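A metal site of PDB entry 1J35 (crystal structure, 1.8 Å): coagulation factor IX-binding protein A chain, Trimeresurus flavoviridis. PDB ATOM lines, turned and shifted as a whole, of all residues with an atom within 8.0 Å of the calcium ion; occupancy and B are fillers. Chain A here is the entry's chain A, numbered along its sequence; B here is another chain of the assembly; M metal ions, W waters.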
ATOM      1  N   TYR A   9      14.428   6.305 -11.486  1.00  0.00           N
ATOM      2  CA  TYR A   9      14.309   6.019 -10.059  1.00  0.00           C
ATOM      3  C   TYR A   9      12.998   6.591  -9.560  1.00  0.00           C
ATOM      4  O   TYR A   9      12.753   7.791  -9.649  1.00  0.00           O
ATOM      5  CB  TYR A   9      15.445   6.639  -9.237  1.00  0.00           C
ATOM      6  CG  TYR A   9      15.292   6.335  -7.755  1.00  0.00           C
ATOM      7  CD1 TYR A   9      15.535   5.050  -7.247  1.00  0.00           C
ATOM      8  CD2 TYR A   9      14.889   7.327  -6.855  1.00  0.00           C
ATOM      9  CE1 TYR A   9      15.405   4.766  -5.884  1.00  0.00           C
ATOM     10  CE2 TYR A   9      14.749   7.053  -5.490  1.00  0.00           C
ATOM     11  CZ  TYR A   9      15.012   5.783  -5.009  1.00  0.00           C
ATOM     12  OH  TYR A   9      14.891   5.521  -3.653  1.00  0.00           O
ATOM     13  N   GLU A  10      12.154   5.710  -9.033  1.00  0.00           N
ATOM     14  CA  GLU A  10      10.865   6.086  -8.482  1.00  0.00           C
ATOM     15  C   GLU A  10      10.104   7.176  -9.234  1.00  0.00           C
ATOM     16  O   GLU A  10       9.893   8.280  -8.724  1.00  0.00           O
ATOM     17  CB  GLU A  10      11.039   6.478  -7.012  1.00  0.00           C
ATOM     18  CG  GLU A  10      11.405   5.274  -6.137  1.00  0.00           C
ATOM     19  CD  GLU A  10      11.449   5.575  -4.646  1.00  0.00           C
ATOM     20  OE1 GLU A  10      11.585   4.607  -3.866  1.00  0.00           O
ATOM     21  OE2 GLU A  10      11.355   6.761  -4.271  1.00  0.00           O
ATOM     22  N   HIS A  12      10.939   9.161 -11.675  1.00  0.00           N
ATOM     23  CA  HIS A  12      11.675  10.262 -12.301  1.00  0.00           C
ATOM     24  C   HIS A  12      12.915   9.763 -13.050  1.00  0.00           C
ATOM     25  O   HIS A  12      13.381   8.661 -12.815  1.00  0.00           O
ATOM     26  CB  HIS A  12      12.072  11.310 -11.253  1.00  0.00           C
ATOM     27  CG  HIS A  12      10.921  11.984 -10.589  1.00  0.00           C
ATOM     28  ND1 HIS A  12      11.070  12.899  -9.570  1.00  0.00           N
ATOM     29  CD2 HIS A  12       9.574  11.868 -10.786  1.00  0.00           C
ATOM     30  CE1 HIS A  12       9.875  13.313  -9.165  1.00  0.00           C
ATOM     31  NE2 HIS A  12       8.958  12.705  -9.885  1.00  0.00           N
ATOM     32  N   CYS A  13      13.419  10.604 -13.952  1.00  0.00           N
ATOM     33  CA  CYS A  13      14.613  10.276 -14.747  1.00  0.00           C
ATOM     34  C   CYS A  13      15.785  11.165 -14.302  1.00  0.00           C
ATOM     35  O   CYS A  13      15.596  12.350 -14.051  1.00  0.00           O
ATOM     36  CB  CYS A  13      14.327  10.521 -16.236  1.00  0.00           C
ATOM     37  SG  CYS A  13      12.978   9.506 -16.915  1.00  0.00           S
ATOM     38  N   TYR A  14      16.979  10.589 -14.211  1.00  0.00           N
ATOM     39  CA  TYR A  14      18.142  11.356 -13.782  1.00  0.00           C
ATOM     40  C   TYR A  14      19.313  11.228 -14.745  1.00  0.00           C
ATOM     41  O   TYR A  14      19.528  10.178 -15.338  1.00  0.00           O
ATOM     42  CB  TYR A  14      18.592  10.892 -12.400  1.00  0.00           C
ATOM     43  CG  TYR A  14      17.509  10.871 -11.340  1.00  0.00           C
ATOM     44  CD1 TYR A  14      16.461   9.958 -11.406  1.00  0.00           C
ATOM     45  CD2 TYR A  14      17.545  11.759 -10.268  1.00  0.00           C
ATOM     46  CE1 TYR A  14      15.477   9.915 -10.427  1.00  0.00           C
ATOM     47  CE2 TYR A  14      16.567  11.721  -9.283  1.00  0.00           C
ATOM     48  CZ  TYR A  14      15.545  10.797  -9.363  1.00  0.00           C
ATOM     49  OH  TYR A  14      14.577  10.749  -8.380  1.00  0.00           O
ATOM     50  N   LEU A  39      17.782  20.996 -11.760  1.00  0.00           N
ATOM     51  CA  LEU A  39      18.893  20.370 -11.047  1.00  0.00           C
ATOM     52  C   LEU A  39      18.195  19.379 -10.119  1.00  0.00           C
ATOM     53  O   LEU A  39      17.047  19.606  -9.732  1.00  0.00           O
ATOM     54  CB  LEU A  39      19.662  21.407 -10.239  1.00  0.00           C
ATOM     55  CG  LEU A  39      20.688  22.199 -11.046  1.00  0.00           C
ATOM     56  CD1 LEU A  39      21.220  23.368 -10.231  1.00  0.00           C
ATOM     57  CD2 LEU A  39      21.818  21.259 -11.461  1.00  0.00           C
ATOM     58  N   VAL A  40      18.875  18.303  -9.773  1.00  0.00           N
ATOM     59  CA  VAL A  40      18.304  17.247  -8.936  1.00  0.00           C
ATOM     60  C   VAL A  40      17.790  17.727  -7.582  1.00  0.00           C
ATOM     61  O   VAL A  40      18.414  18.523  -6.903  1.00  0.00           O
ATOM     62  CB  VAL A  40      19.343  16.102  -8.722  1.00  0.00           C
ATOM     63  CG1 VAL A  40      20.537  16.601  -7.926  1.00  0.00           C
ATOM     64  CG2 VAL A  40      18.685  14.896  -8.049  1.00  0.00           C
ATOM     65  N   SER A  41      16.616  17.238  -7.199  1.00  0.00           N
ATOM     66  CA  SER A  41      16.032  17.561  -5.903  1.00  0.00           C
ATOM     67  C   SER A  41      16.077  16.263  -5.108  1.00  0.00           C
ATOM     68  O   SER A  41      15.476  15.271  -5.505  1.00  0.00           O
ATOM     69  CB  SER A  41      14.584  18.061  -6.070  1.00  0.00           C
ATOM     70  OG  SER A  41      13.768  17.113  -6.752  1.00  0.00           O
ATOM     71  N   ILE A  42      16.818  16.265  -4.008  1.00  0.00           N
ATOM     72  CA  ILE A  42      16.995  15.087  -3.169  1.00  0.00           C
ATOM     73  C   ILE A  42      15.986  15.129  -2.036  1.00  0.00           C
ATOM     74  O   ILE A  42      16.179  15.813  -1.033  1.00  0.00           O
ATOM     75  CB  ILE A  42      18.439  15.046  -2.646  1.00  0.00           C
ATOM     76  CG1 ILE A  42      19.400  15.008  -3.844  1.00  0.00           C
ATOM     77  CG2 ILE A  42      18.650  13.823  -1.776  1.00  0.00           C
ATOM     78  CD1 ILE A  42      20.868  14.888  -3.463  1.00  0.00           C
ATOM     79  N   GLU A  43      14.901  14.368  -2.216  1.00  0.00           N
ATOM     80  CA  GLU A  43      13.787  14.350  -1.261  1.00  0.00           C
ATOM     81  C   GLU A  43      13.630  13.185  -0.301  1.00  0.00           C
ATOM     82  O   GLU A  43      12.634  13.110   0.434  1.00  0.00           O
ATOM     83  CB  GLU A  43      12.490  14.529  -2.037  1.00  0.00           C
ATOM     84  CG  GLU A  43      12.394  15.860  -2.754  1.00  0.00           C
ATOM     85  CD  GLU A  43      11.533  15.791  -3.987  1.00  0.00           C
ATOM     86  OE1 GLU A  43      12.086  15.505  -5.079  1.00  0.00           O
ATOM     87  OE2 GLU A  43      10.311  16.001  -3.875  1.00  0.00           O
ATOM     88  N   SER A  44      14.581  12.263  -0.292  1.00  0.00           N
ATOM     89  CA  SER A  44      14.531  11.122   0.608  1.00  0.00           C
ATOM     90  C   SER A  44      15.907  10.497   0.611  1.00  0.00           C
ATOM     91  O   SER A  44      16.696  10.745  -0.298  1.00  0.00           O
ATOM     92  CB  SER A  44      13.487  10.101   0.146  1.00  0.00           C
ATOM     93  OG  SER A  44      13.806   9.563  -1.126  1.00  0.00           O
ATOM     94  N   GLU A  47      16.533   8.302  -2.554  1.00  0.00           N
ATOM     95  CA  GLU A  47      16.872   9.080  -3.730  1.00  0.00           C
ATOM     96  C   GLU A  47      18.307   9.593  -3.575  1.00  0.00           C
ATOM     97  O   GLU A  47      19.050   9.679  -4.544  1.00  0.00           O
ATOM     98  CB  GLU A  47      15.890  10.247  -3.903  1.00  0.00           C
ATOM     99  CG  GLU A  47      16.156  11.113  -5.119  1.00  0.00           C
ATOM    100  CD  GLU A  47      15.086  12.180  -5.314  1.00  0.00           C
ATOM    101  OE1 GLU A  47      14.462  12.582  -4.326  1.00  0.00           O
ATOM    102  OE2 GLU A  47      14.895  12.619  -6.470  1.00  0.00           O
ATOM    103  N   VAL A  51      21.211   8.849  -6.295  1.00  0.00           N
ATOM    104  CA  VAL A  51      21.987   9.935  -6.901  1.00  0.00           C
ATOM    105  C   VAL A  51      23.485   9.809  -6.628  1.00  0.00           C
ATOM    106  O   VAL A  51      24.304  10.056  -7.531  1.00  0.00           O
ATOM    107  CB  VAL A  51      21.503  11.308  -6.414  1.00  0.00           C
ATOM    108  CG1 VAL A  51      22.407  12.422  -6.954  1.00  0.00           C
ATOM    109  CG2 VAL A  51      20.060  11.512  -6.870  1.00  0.00           C
ATOM    110  N   GLU A 128      17.324  16.358 -13.171  1.00  0.00           N
ATOM    111  CA  GLU A 128      16.203  15.492 -12.860  1.00  0.00           C
ATOM    112  C   GLU A 128      14.943  15.940 -13.582  1.00  0.00           C
ATOM    113  O   GLU A 128      14.679  17.140 -13.712  1.00  0.00           O
ATOM    114  CB  GLU A 128      15.933  15.464 -11.346  1.00  0.00           C
ATOM    115  CG  GLU A 128      14.755  14.548 -10.986  1.00  0.00           C
ATOM    116  CD  GLU A 128      14.414  14.545  -9.503  1.00  0.00           C
ATOM    117  OE1 GLU A 128      13.469  13.820  -9.125  1.00  0.00           O
ATOM    118  OE2 GLU A 128      15.077  15.258  -8.730  1.00  0.00           O
ATOM    119  N   ALA A 129      14.171  14.972 -14.056  1.00  0.00           N
ATOM    120  CA  ALA A 129      12.917  15.238 -14.736  1.00  0.00           C
ATOM    121  C   ALA A 129      11.941  14.160 -14.276  1.00  0.00           C
ATOM    122  O   ALA A 129      12.322  12.971 -14.291  1.00  0.00           O
ATOM    123  CB  ALA A 129      13.114  15.158 -16.250  1.00  0.00           C
ATOM    124  OXT ALA A 129      10.819  14.526 -13.870  1.00  0.00           O
ATOM    125  N   TRP B  79      13.835  24.240  -3.502  1.00  0.00           N
ATOM    126  CA  TRP B  79      14.296  23.394  -4.588  1.00  0.00           C
ATOM    127  C   TRP B  79      13.887  24.111  -5.878  1.00  0.00           C
ATOM    128  O   TRP B  79      12.816  24.709  -5.940  1.00  0.00           O
ATOM    129  CB  TRP B  79      13.640  22.004  -4.534  1.00  0.00           C
ATOM    130  CG  TRP B  79      14.148  21.108  -3.426  1.00  0.00           C
ATOM    131  CD1 TRP B  79      13.453  20.716  -2.312  1.00  0.00           C
ATOM    132  CD2 TRP B  79      15.446  20.505  -3.329  1.00  0.00           C
ATOM    133  NE1 TRP B  79      14.240  19.896  -1.524  1.00  0.00           N
ATOM    134  CE2 TRP B  79      15.467  19.749  -2.131  1.00  0.00           C
ATOM    135  CE3 TRP B  79      16.583  20.515  -4.138  1.00  0.00           C
ATOM    136  CZ2 TRP B  79      16.588  19.025  -1.724  1.00  0.00           C
ATOM    137  CZ3 TRP B  79      17.706  19.782  -3.727  1.00  0.00           C
ATOM    138  CH2 TRP B  79      17.699  19.050  -2.534  1.00  0.00           C
ATOM    139  N   ASN B  81      12.913  22.832  -8.561  1.00  0.00           N
ATOM    140  CA  ASN B  81      11.751  22.178  -9.167  1.00  0.00           C
ATOM    141  C   ASN B  81      10.506  22.439  -8.316  1.00  0.00           C
ATOM    142  O   ASN B  81       9.442  21.885  -8.574  1.00  0.00           O
ATOM    143  CB  ASN B  81      11.990  20.682  -9.285  1.00  0.00           C
ATOM    144  CG  ASN B  81      11.781  19.961  -7.978  1.00  0.00           C
ATOM    145  OD1 ASN B  81      12.142  20.455  -6.917  1.00  0.00           O
ATOM    146  ND2 ASN B  81      11.190  18.760  -8.043  1.00  0.00           N
ATOM    147  N   ALA B  83       9.875  21.455  -5.305  1.00  0.00           N
ATOM    148  CA  ALA B  83       9.459  20.386  -4.412  1.00  0.00           C
ATOM    149  C   ALA B  83       9.556  20.958  -2.996  1.00  0.00           C
ATOM    150  O   ALA B  83      10.384  21.825  -2.734  1.00  0.00           O
ATOM    151  CB  ALA B  83      10.398  19.184  -4.572  1.00  0.00           C
HETATM  152 CA    CA M   1      13.486  14.572  -6.777  1.00  0.00          CA
HETATM  153  O   HOH W   1      11.867  12.948  -6.621  1.00  0.00           O
HETATM  154  O   HOH W   2      11.702  15.706  -8.210  1.00  0.00           O
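The calcium ion is bound by water W1 (2.3 Å), the side-chain carboxylate (OE1) of Glu 43 (2.4 Å), the side-chain carboxylate (OE2) of Glu 47 (2.4 Å), the backbone carbonyl oxygen (O) of Ser 41 (2.5 Å), the side-chain carboxylate (OE1) of Glu 128 (2.5 Å), water W2 (2.6 Å), the side-chain hydroxyl (OG) of Ser 41 (2.6 Å) and the side-chain carboxylate (OE2) of Glu 128 (2.6 Å).
Water W1 bridges ND1 of His 12 (3.1 Å) and OE1 of Glu 47 (3.5 Å).
Water W2 bridges ND2 of Asn 81 of chain B (3.1 Å) and ND1 of His 12 (3.2 Å).
The side-chain carboxylate of Glu 47 lies close to the side-chain hydroxyl of Tyr 14.
The side-chain hydroxyl of Ser 44 is in hydrogen-bond range of the backbone NH of Glu 47.
The backbone NH (N) of Glu 47 sits at hydrogen-bond distance from the side-chain hydroxyl (OH) of Tyr 9.
OG of Ser 41 sits close to ND2 of Asn 81 of chain B, 3.3 Å away.
OE1 of Glu 128 lies close to ND1 of His 12, at 2.6 Å.
The side-chain carboxylate of Glu 128 sits close to the side-chain hydroxyl of Tyr 14 (3.3 Å).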
